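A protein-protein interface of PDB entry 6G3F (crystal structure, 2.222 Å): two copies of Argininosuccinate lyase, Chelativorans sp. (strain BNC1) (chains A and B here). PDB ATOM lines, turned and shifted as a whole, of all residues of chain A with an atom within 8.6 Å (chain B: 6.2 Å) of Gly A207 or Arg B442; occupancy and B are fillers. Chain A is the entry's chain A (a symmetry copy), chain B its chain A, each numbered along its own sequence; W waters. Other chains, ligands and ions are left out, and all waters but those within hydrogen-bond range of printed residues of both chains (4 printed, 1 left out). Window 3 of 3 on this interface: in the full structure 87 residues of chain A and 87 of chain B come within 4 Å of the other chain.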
ATOM      1  N   ILE A  59     -20.414 -14.430   7.059  1.00  0.00           N
ATOM      2  CA  ILE A  59     -20.649 -14.976   5.727  1.00  0.00           C
ATOM      3  C   ILE A  59     -21.026 -13.878   4.738  1.00  0.00           C
ATOM      4  O   ILE A  59     -20.673 -13.964   3.558  1.00  0.00           O
ATOM      5  CB  ILE A  59     -21.735 -16.063   5.792  1.00  0.00           C
ATOM      6  CG1 ILE A  59     -21.242 -17.238   6.635  1.00  0.00           C
ATOM      7  CG2 ILE A  59     -22.119 -16.547   4.389  1.00  0.00           C
ATOM      8  CD1 ILE A  59     -22.344 -18.134   7.138  1.00  0.00           C
ATOM      9  N   ILE A 108     -27.667 -18.497   0.986  1.00  0.00           N
ATOM     10  CA  ILE A 108     -26.517 -19.295   1.399  1.00  0.00           C
ATOM     11  C   ILE A 108     -26.901 -20.158   2.590  1.00  0.00           C
ATOM     12  O   ILE A 108     -27.472 -19.672   3.573  1.00  0.00           O
ATOM     13  CB  ILE A 108     -25.323 -18.387   1.733  1.00  0.00           C
ATOM     14  CG1 ILE A 108     -24.735 -17.793   0.451  1.00  0.00           C
ATOM     15  CG2 ILE A 108     -24.237 -19.163   2.490  1.00  0.00           C
ATOM     16  CD1 ILE A 108     -23.723 -16.695   0.694  1.00  0.00           C
ATOM     17  N   GLY A 109     -26.574 -21.447   2.509  1.00  0.00           N
ATOM     18  CA  GLY A 109     -26.848 -22.360   3.601  1.00  0.00           C
ATOM     19  C   GLY A 109     -28.316 -22.610   3.848  1.00  0.00           C
ATOM     20  O   GLY A 109     -28.691 -23.007   4.954  1.00  0.00           O
ATOM     21  N   ARG A 110     -29.161 -22.401   2.842  1.00  0.00           N
ATOM     22  CA  ARG A 110     -30.601 -22.438   3.025  1.00  0.00           C
ATOM     23  C   ARG A 110     -31.254 -23.081   1.811  1.00  0.00           C
ATOM     24  O   ARG A 110     -30.669 -23.160   0.727  1.00  0.00           O
ATOM     25  CB  ARG A 110     -31.153 -21.026   3.250  1.00  0.00           C
ATOM     26  CG  ARG A 110     -32.576 -20.976   3.762  1.00  0.00           C
ATOM     27  CD  ARG A 110     -33.009 -19.541   3.998  1.00  0.00           C
ATOM     28  NE  ARG A 110     -33.052 -18.780   2.753  1.00  0.00           N
ATOM     29  CZ  ARG A 110     -33.511 -17.537   2.650  1.00  0.00           C
ATOM     30  NH1 ARG A 110     -33.972 -16.906   3.721  1.00  0.00           N
ATOM     31  NH2 ARG A 110     -33.516 -16.925   1.471  1.00  0.00           N
ATOM     32  N   GLY A 199     -31.687 -24.043   9.224  1.00  0.00           N
ATOM     33  CA  GLY A 199     -30.383 -24.653   9.353  1.00  0.00           C
ATOM     34  C   GLY A 199     -30.322 -26.049   8.778  1.00  0.00           C
ATOM     35  O   GLY A 199     -29.223 -26.539   8.485  1.00  0.00           O
ATOM     36  N   ALA A 201     -31.466 -26.708   5.878  1.00  0.00           N
ATOM     37  CA  ALA A 201     -31.300 -26.472   4.440  1.00  0.00           C
ATOM     38  C   ALA A 201     -32.159 -27.494   3.695  1.00  0.00           C
ATOM     39  O   ALA A 201     -33.357 -27.606   3.989  1.00  0.00           O
ATOM     40  CB  ALA A 201     -29.819 -26.487   4.097  1.00  0.00           C
ATOM     41  N   ALA A 204     -30.049 -32.003   4.944  1.00  0.00           N
ATOM     42  CA  ALA A 204     -28.811 -32.513   5.523  1.00  0.00           C
ATOM     43  C   ALA A 204     -27.949 -31.411   6.128  1.00  0.00           C
ATOM     44  O   ALA A 204     -26.759 -31.627   6.374  1.00  0.00           O
ATOM     45  CB  ALA A 204     -28.014 -33.277   4.464  1.00  0.00           C
ATOM     46  N   GLY A 205     -28.517 -30.233   6.376  1.00  0.00           N
ATOM     47  CA  GLY A 205     -27.714 -29.141   6.892  1.00  0.00           C
ATOM     48  C   GLY A 205     -26.832 -28.543   5.808  1.00  0.00           C
ATOM     49  O   GLY A 205     -27.154 -28.571   4.616  1.00  0.00           O
ATOM     50  N   THR A 206     -25.693 -27.995   6.231  1.00  0.00           N
ATOM     51  CA  THR A 206     -24.813 -27.285   5.312  1.00  0.00           C
ATOM     52  C   THR A 206     -23.408 -27.218   5.890  1.00  0.00           C
ATOM     53  O   THR A 206     -23.202 -27.352   7.100  1.00  0.00           O
ATOM     54  CB  THR A 206     -25.331 -25.868   5.026  1.00  0.00           C
ATOM     55  OG1 THR A 206     -24.403 -25.173   4.182  1.00  0.00           O
ATOM     56  CG2 THR A 206     -25.501 -25.087   6.322  1.00  0.00           C
ATOM     57  N   GLY A 207     -22.437 -26.997   5.000  1.00  0.00           N
ATOM     58  CA  GLY A 207     -21.077 -26.731   5.431  1.00  0.00           C
ATOM     59  C   GLY A 207     -20.861 -25.323   5.939  1.00  0.00           C
ATOM     60  O   GLY A 207     -19.889 -25.077   6.658  1.00  0.00           O
ATOM     61  N   TRP A 208     -21.747 -24.398   5.585  1.00  0.00           N
ATOM     62  CA  TRP A 208     -21.625 -23.035   6.075  1.00  0.00           C
ATOM     63  C   TRP A 208     -21.827 -23.007   7.588  1.00  0.00           C
ATOM     64  O   TRP A 208     -22.710 -23.696   8.109  1.00  0.00           O
ATOM     65  CB  TRP A 208     -22.642 -22.123   5.394  1.00  0.00           C
ATOM     66  CG  TRP A 208     -22.350 -21.895   3.946  1.00  0.00           C
ATOM     67  CD1 TRP A 208     -22.911 -22.542   2.887  1.00  0.00           C
ATOM     68  CD2 TRP A 208     -21.417 -20.955   3.394  1.00  0.00           C
ATOM     69  NE1 TRP A 208     -22.389 -22.064   1.709  1.00  0.00           N
ATOM     70  CE2 TRP A 208     -21.470 -21.090   1.992  1.00  0.00           C
ATOM     71  CE3 TRP A 208     -20.544 -20.013   3.949  1.00  0.00           C
ATOM     72  CZ2 TRP A 208     -20.686 -20.315   1.136  1.00  0.00           C
ATOM     73  CZ3 TRP A 208     -19.766 -19.245   3.097  1.00  0.00           C
ATOM     74  CH2 TRP A 208     -19.842 -19.403   1.707  1.00  0.00           C
ATOM     75  N   PRO A 209     -21.000 -22.199   8.347  1.00  0.00           N
ATOM     76  CA  PRO A 209     -21.112 -22.179   9.820  1.00  0.00           C
ATOM     77  C   PRO A 209     -22.263 -21.307  10.320  1.00  0.00           C
ATOM     78  O   PRO A 209     -22.097 -20.195  10.826  1.00  0.00           O
ATOM     79  CB  PRO A 209     -19.748 -21.637  10.250  1.00  0.00           C
ATOM     80  CG  PRO A 209     -19.330 -20.752   9.127  1.00  0.00           C
ATOM     81  CD  PRO A 209     -19.896 -21.352   7.865  1.00  0.00           C
ATOM     82  N   LEU A 210     -23.478 -21.832  10.181  1.00  0.00           N
ATOM     83  CA  LEU A 210     -24.663 -21.124  10.639  1.00  0.00           C
ATOM     84  C   LEU A 210     -24.766 -21.183  12.156  1.00  0.00           C
ATOM     85  O   LEU A 210     -24.308 -22.133  12.797  1.00  0.00           O
ATOM     86  CB  LEU A 210     -25.931 -21.725  10.030  1.00  0.00           C
ATOM     87  CG  LEU A 210     -25.958 -21.988   8.523  1.00  0.00           C
ATOM     88  CD1 LEU A 210     -27.368 -22.365   8.093  1.00  0.00           C
ATOM     89  CD2 LEU A 210     -25.455 -20.787   7.732  1.00  0.00           C
ATOM     90  N   ASP B 369     -22.075 -28.944  -2.448  1.00  0.00           N
ATOM     91  CA  ASP B 369     -20.771 -28.554  -1.920  1.00  0.00           C
ATOM     92  C   ASP B 369     -19.911 -27.925  -3.006  1.00  0.00           C
ATOM     93  O   ASP B 369     -19.176 -26.964  -2.747  1.00  0.00           O
ATOM     94  CB  ASP B 369     -20.069 -29.762  -1.299  1.00  0.00           C
ATOM     95  CG  ASP B 369     -20.416 -29.947   0.167  1.00  0.00           C
ATOM     96  OD1 ASP B 369     -21.450 -29.402   0.608  1.00  0.00           O
ATOM     97  OD2 ASP B 369     -19.656 -30.636   0.882  1.00  0.00           O
ATOM     98  N   ASP B 372     -21.350 -24.443  -3.201  1.00  0.00           N
ATOM     99  CA  ASP B 372     -20.915 -23.667  -2.043  1.00  0.00           C
ATOM    100  C   ASP B 372     -19.447 -23.273  -2.162  1.00  0.00           C
ATOM    101  O   ASP B 372     -19.055 -22.177  -1.747  1.00  0.00           O
ATOM    102  CB  ASP B 372     -21.139 -24.466  -0.755  1.00  0.00           C
ATOM    103  CG  ASP B 372     -22.606 -24.564  -0.359  1.00  0.00           C
ATOM    104  OD1 ASP B 372     -23.396 -23.672  -0.726  1.00  0.00           O
ATOM    105  OD2 ASP B 372     -22.964 -25.533   0.342  1.00  0.00           O
ATOM    106  N   ARG B 376     -17.843 -19.570  -1.877  1.00  0.00           N
ATOM    107  CA  ARG B 376     -16.868 -19.298  -0.830  1.00  0.00           C
ATOM    108  C   ARG B 376     -15.543 -18.811  -1.408  1.00  0.00           C
ATOM    109  O   ARG B 376     -14.922 -17.893  -0.862  1.00  0.00           O
ATOM    110  CB  ARG B 376     -16.657 -20.569  -0.017  1.00  0.00           C
ATOM    111  CG  ARG B 376     -15.920 -20.405   1.309  1.00  0.00           C
ATOM    112  CD  ARG B 376     -15.650 -21.763   1.953  1.00  0.00           C
ATOM    113  NE  ARG B 376     -15.201 -22.751   0.974  1.00  0.00           N
ATOM    114  CZ  ARG B 376     -14.897 -24.016   1.252  1.00  0.00           C
ATOM    115  NH1 ARG B 376     -14.986 -24.489   2.489  1.00  0.00           N
ATOM    116  NH2 ARG B 376     -14.503 -24.816   0.272  1.00  0.00           N
ATOM    117  N   ASP B 432     -11.973 -32.003  -3.293  1.00  0.00           N
ATOM    118  CA  ASP B 432     -12.468 -31.986  -1.922  1.00  0.00           C
ATOM    119  C   ASP B 432     -13.972 -31.747  -1.876  1.00  0.00           C
ATOM    120  O   ASP B 432     -14.664 -32.302  -1.015  1.00  0.00           O
ATOM    121  CB  ASP B 432     -11.727 -30.910  -1.125  1.00  0.00           C
ATOM    122  CG  ASP B 432     -12.119 -30.889   0.339  1.00  0.00           C
ATOM    123  OD1 ASP B 432     -12.345 -31.973   0.917  1.00  0.00           O
ATOM    124  OD2 ASP B 432     -12.194 -29.783   0.916  1.00  0.00           O
ATOM    125  N   ALA B 433     -14.497 -30.932  -2.795  1.00  0.00           N
ATOM    126  CA  ALA B 433     -15.926 -30.642  -2.803  1.00  0.00           C
ATOM    127  C   ALA B 433     -16.745 -31.860  -3.206  1.00  0.00           C
ATOM    128  O   ALA B 433     -17.876 -32.027  -2.736  1.00  0.00           O
ATOM    129  CB  ALA B 433     -16.219 -29.478  -3.748  1.00  0.00           C
ATOM    130  N   LEU B 434     -16.197 -32.716  -4.065  1.00  0.00           N
ATOM    131  CA  LEU B 434     -16.914 -33.873  -4.580  1.00  0.00           C
ATOM    132  C   LEU B 434     -16.671 -35.135  -3.767  1.00  0.00           C
ATOM    133  O   LEU B 434     -17.189 -36.196  -4.128  1.00  0.00           O
ATOM    134  CB  LEU B 434     -16.521 -34.120  -6.038  1.00  0.00           C
ATOM    135  CG  LEU B 434     -16.827 -32.952  -6.977  1.00  0.00           C
ATOM    136  CD1 LEU B 434     -16.287 -33.225  -8.371  1.00  0.00           C
ATOM    137  CD2 LEU B 434     -18.318 -32.688  -7.027  1.00  0.00           C
ATOM    138  N   ASP B 435     -15.905 -35.048  -2.688  1.00  0.00           N
ATOM    139  CA  ASP B 435     -15.673 -36.196  -1.825  1.00  0.00           C
ATOM    140  C   ASP B 435     -16.862 -36.352  -0.883  1.00  0.00           C
ATOM    141  O   ASP B 435     -17.048 -35.519   0.015  1.00  0.00           O
ATOM    142  CB  ASP B 435     -14.374 -36.018  -1.039  1.00  0.00           C
ATOM    143  CG  ASP B 435     -14.007 -37.248  -0.232  1.00  0.00           C
ATOM    144  OD1 ASP B 435     -14.899 -37.821   0.429  1.00  0.00           O
ATOM    145  OD2 ASP B 435     -12.824 -37.643  -0.261  1.00  0.00           O
ATOM    146  N   TRP B 437     -17.543 -38.147   1.698  1.00  0.00           N
ATOM    147  CA  TRP B 437     -17.253 -38.192   3.127  1.00  0.00           C
ATOM    148  C   TRP B 437     -16.909 -36.806   3.657  1.00  0.00           C
ATOM    149  O   TRP B 437     -17.286 -36.455   4.782  1.00  0.00           O
ATOM    150  CB  TRP B 437     -16.120 -39.175   3.412  1.00  0.00           C
ATOM    151  CG  TRP B 437     -15.833 -39.312   4.876  1.00  0.00           C
ATOM    152  CD1 TRP B 437     -14.653 -39.054   5.509  1.00  0.00           C
ATOM    153  CD2 TRP B 437     -16.754 -39.720   5.893  1.00  0.00           C
ATOM    154  NE1 TRP B 437     -14.779 -39.286   6.859  1.00  0.00           N
ATOM    155  CE2 TRP B 437     -16.060 -39.697   7.120  1.00  0.00           C
ATOM    156  CE3 TRP B 437     -18.097 -40.111   5.885  1.00  0.00           C
ATOM    157  CZ2 TRP B 437     -16.664 -40.046   8.326  1.00  0.00           C
ATOM    158  CZ3 TRP B 437     -18.695 -40.459   7.084  1.00  0.00           C
ATOM    159  CH2 TRP B 437     -17.979 -40.423   8.287  1.00  0.00           C
ATOM    160  N   GLN B 438     -16.199 -36.001   2.862  1.00  0.00           N
ATOM    161  CA  GLN B 438     -15.952 -34.616   3.251  1.00  0.00           C
ATOM    162  C   GLN B 438     -17.244 -33.811   3.269  1.00  0.00           C
ATOM    163  O   GLN B 438     -17.398 -32.909   4.098  1.00  0.00           O
ATOM    164  CB  GLN B 438     -14.935 -33.973   2.306  1.00  0.00           C
ATOM    165  CG  GLN B 438     -13.595 -34.693   2.258  1.00  0.00           C
ATOM    166  CD  GLN B 438     -12.933 -34.788   3.619  1.00  0.00           C
ATOM    167  OE1 GLN B 438     -12.827 -33.798   4.342  1.00  0.00           O
ATOM    168  NE2 GLN B 438     -12.496 -35.988   3.981  1.00  0.00           N
ATOM    169  N   ASN B 439     -18.178 -34.116   2.363  1.00  0.00           N
ATOM    170  CA  ASN B 439     -19.509 -33.521   2.443  1.00  0.00           C
ATOM    171  C   ASN B 439     -20.125 -33.763   3.813  1.00  0.00           C
ATOM    172  O   ASN B 439     -20.693 -32.849   4.423  1.00  0.00           O
ATOM    173  CB  ASN B 439     -20.415 -34.097   1.353  1.00  0.00           C
ATOM    174  CG  ASN B 439     -20.270 -33.386   0.026  1.00  0.00           C
ATOM    175  OD1 ASN B 439     -21.204 -32.741  -0.451  1.00  0.00           O
ATOM    176  ND2 ASN B 439     -19.099 -33.512  -0.585  1.00  0.00           N
ATOM    177  N   VAL B 440     -20.018 -34.995   4.313  1.00  0.00           N
ATOM    178  CA  VAL B 440     -20.566 -35.328   5.624  1.00  0.00           C
ATOM    179  C   VAL B 440     -19.813 -34.587   6.722  1.00  0.00           C
ATOM    180  O   VAL B 440     -20.421 -33.964   7.602  1.00  0.00           O
ATOM    181  CB  VAL B 440     -20.529 -36.853   5.840  1.00  0.00           C
ATOM    182  CG1 VAL B 440     -20.865 -37.220   7.284  1.00  0.00           C
ATOM    183  CG2 VAL B 440     -21.493 -37.542   4.881  1.00  0.00           C
ATOM    184  N   LEU B 441     -18.479 -34.637   6.687  1.00  0.00           N
ATOM    185  CA  LEU B 441     -17.688 -34.035   7.758  1.00  0.00           C
ATOM    186  C   LEU B 441     -17.950 -32.540   7.866  1.00  0.00           C
ATOM    187  O   LEU B 441     -17.967 -31.981   8.968  1.00  0.00           O
ATOM    188  CB  LEU B 441     -16.200 -34.293   7.527  1.00  0.00           C
ATOM    189  CG  LEU B 441     -15.741 -35.749   7.637  1.00  0.00           C
ATOM    190  CD1 LEU B 441     -14.269 -35.860   7.280  1.00  0.00           C
ATOM    191  CD2 LEU B 441     -15.996 -36.299   9.033  1.00  0.00           C
ATOM    192  N   ARG B 442     -18.157 -31.875   6.732  1.00  0.00           N
ATOM    193  CA  ARG B 442     -18.368 -30.435   6.765  1.00  0.00           C
ATOM    194  C   ARG B 442     -19.717 -30.071   7.366  1.00  0.00           C
ATOM    195  O   ARG B 442     -19.878 -28.970   7.903  1.00  0.00           O
ATOM    196  CB  ARG B 442     -18.237 -29.870   5.357  1.00  0.00           C
ATOM    197  CG  ARG B 442     -16.807 -29.869   4.840  1.00  0.00           C
ATOM    198  CD  ARG B 442     -16.741 -29.146   3.537  1.00  0.00           C
ATOM    199  NE  ARG B 442     -17.151 -29.982   2.409  1.00  0.00           N
ATOM    200  CZ  ARG B 442     -16.321 -30.616   1.583  1.00  0.00           C
ATOM    201  NH1 ARG B 442     -15.007 -30.522   1.731  1.00  0.00           N
ATOM    202  NH2 ARG B 442     -16.807 -31.354   0.591  1.00  0.00           N
ATOM    203  N   ARG B 443     -20.692 -30.977   7.292  1.00  0.00           N
ATOM    204  CA  ARG B 443     -22.011 -30.743   7.875  1.00  0.00           C
ATOM    205  C   ARG B 443     -21.971 -31.175   9.336  1.00  0.00           C
ATOM    206  O   ARG B 443     -22.433 -32.251   9.720  1.00  0.00           O
ATOM    207  CB  ARG B 443     -23.074 -31.489   7.082  1.00  0.00           C
ATOM    208  CG  ARG B 443     -23.371 -30.857   5.739  1.00  0.00           C
ATOM    209  CD  ARG B 443     -24.018 -31.833   4.777  1.00  0.00           C
ATOM    210  NE  ARG B 443     -24.443 -31.146   3.563  1.00  0.00           N
ATOM    211  CZ  ARG B 443     -23.638 -30.854   2.546  1.00  0.00           C
ATOM    212  NH1 ARG B 443     -24.114 -30.213   1.488  1.00  0.00           N
ATOM    213  NH2 ARG B 443     -22.358 -31.202   2.583  1.00  0.00           N
ATOM    214  N   GLU B 444     -21.410 -30.295  10.170  1.00  0.00           N
ATOM    215  CA  GLU B 444     -21.103 -30.622  11.557  1.00  0.00           C
ATOM    216  C   GLU B 444     -21.861 -29.760  12.560  1.00  0.00           C
ATOM    217  O   GLU B 444     -21.603 -29.866  13.764  1.00  0.00           O
ATOM    218  CB  GLU B 444     -19.595 -30.498  11.796  1.00  0.00           C
ATOM    219  CG  GLU B 444     -19.026 -29.128  11.466  1.00  0.00           C
ATOM    220  CD  GLU B 444     -17.564 -29.003  11.839  1.00  0.00           C
ATOM    221  OE1 GLU B 444     -16.945 -30.037  12.167  1.00  0.00           O
ATOM    222  OE2 GLU B 444     -17.036 -27.871  11.805  1.00  0.00           O
ATOM    223  N   GLY B 445     -22.783 -28.918  12.109  1.00  0.00           N
ATOM    224  CA  GLY B 445     -23.626 -28.184  13.024  1.00  0.00           C
ATOM    225  C   GLY B 445     -24.644 -29.095  13.695  1.00  0.00           C
ATOM    226  O   GLY B 445     -24.657 -30.314  13.526  1.00  0.00           O
ATOM    227  N   MET B 448     -26.784 -32.317  12.102  1.00  0.00           N
ATOM    228  CA  MET B 448     -26.211 -32.608  10.799  1.00  0.00           C
ATOM    229  C   MET B 448     -25.450 -33.931  10.837  1.00  0.00           C
ATOM    230  O   MET B 448     -25.139 -34.448  11.914  1.00  0.00           O
ATOM    231  CB  MET B 448     -25.298 -31.450  10.377  1.00  0.00           C
ATOM    232  CG  MET B 448     -26.018 -30.097  10.414  1.00  0.00           C
ATOM    233  SD  MET B 448     -25.094 -28.730   9.681  1.00  0.00           S
ATOM    234  CE  MET B 448     -26.152 -27.344  10.082  1.00  0.00           C
ATOM    235  N   ALA B 450     -22.478 -35.157  10.389  1.00  0.00           N
ATOM    236  CA  ALA B 450     -21.105 -35.406  10.809  1.00  0.00           C
ATOM    237  C   ALA B 450     -21.096 -36.308  12.044  1.00  0.00           C
ATOM    238  O   ALA B 450     -21.919 -36.124  12.949  1.00  0.00           O
ATOM    239  CB  ALA B 450     -20.383 -34.094  11.114  1.00  0.00           C
HETATM  240  O   HOH W   1     -21.988 -27.235   2.258  1.00  0.00           O
HETATM  241  O   HOH W   2     -25.194 -25.534   1.755  1.00  0.00           O
HETATM  242  O   HOH W   3     -26.308 -28.090   2.062  1.00  0.00           O
HETATM  243  O   HOH W   4     -25.911 -23.249   0.495  1.00  0.00           O
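OD1 of Asp B372 lies within hydrogen-bond range of NE1 of Trp A208 (3.1 Å). The backbone NH (N) of Thr A206 is in hydrogen-bond range of the side-chain sulfur (SD) of Met B448 (3.6 Å).
Water W2 bridges the side-chain hydroxyl of Thr A206 (2.6 Å) and the side-chain carboxylate of Asp B372 (2.6 Å). Water W3 lies within hydrogen-bond range of the backbone carbonyl oxygen of Gly A205 (2.7 Å) and the guanidinium group of Arg B443 (3.1 Å). Water W1 lies within hydrogen-bond range of the side-chain carboxylate (OD2) of Asp B372 (2.7 Å), the side-chain carboxylate (OD1) of Asp B369 (2.8 Å) and the backbone NH (N) of Gly A207 (2.8 Å). Water W4 bridges N of Gly A109 and OD1 of Asp B372.
Of the 18 printed residues of chain B, 5 touch a printed residue of chain A. Hydrophobic or aromatic side chains of chain B within 4 Å of the printed part of chain A: Met B448. Among the printed residues, 10 pairs touch across the chains. Among the printed residues, no Asp or Glu carboxylate lies within 4 Å of a Lys or Arg side-chain nitrogen of the other chain.
Among the printed residues, pairs that only touch across the chains: Ala A204 with Arg B443 (3.2 Å), Gly A207 with Arg B442 (3.5 Å), Gly A199 with Met B448 (3.6 Å), Thr A206 with Arg B443 (3.6 Å), Thr A206 with Arg B442 (3.8 Å), Trp A208 with Arg B376 (3.8 Å), Gly A205 with Met B448 (3.8 Å) and Gly A205 with Arg B443 (3.9 Å).
Of chain B, only Arg B442 (3.5 Å) comes within 4 Å of Gly A207. Of chain A, only Thr A206 (3.8 Å) and Gly A207 (3.5 Å) come within 4 Å of Arg B442. Printed residues of chain A within 4 Å of Met B448: Gly A199, Gly A205 and Thr A206. Of the printed residues of chain B, Thr A206 touches Arg B442 (3.8 Å), Arg B443 (3.6 Å) and Met B448 (3.5 Å). Of the printed residues of chain B, Gly A199 touches Met B448 (3.6 Å). Printed residues of chain B within 4 Å of Trp A208: Asp B372 and Arg B376. The nearest residue of chain B that does not touch Gly A207 is Arg B443 (4.04 Å).
The guanidinium group (NH1) of Arg B442 is in salt-bridge range of the side-chain carboxylate (OD2) of Asp B432 (3.0 Å). The backbone carbonyl oxygen (O) of Gln B438 lies close to the guanidinium group (NE) of Arg B442 (3.4 Å). The side-chain amide nitrogen of Asn B439 sits close to the guanidinium group of Arg B442. The backbone carbonyl oxygen (O) of Asn B439 sits at hydrogen-bond distance from the guanidinium group (NH2) of Arg B443, 3.0 Å away. The backbone carbonyl oxygen of Arg B443 sits at hydrogen-bond distance from the backbone NH of Ala B450 (3.0 Å). OG1 of Thr A206 lies within hydrogen-bond range of N of Trp A208, 3.1 Å away.
No position is printed for both chains.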
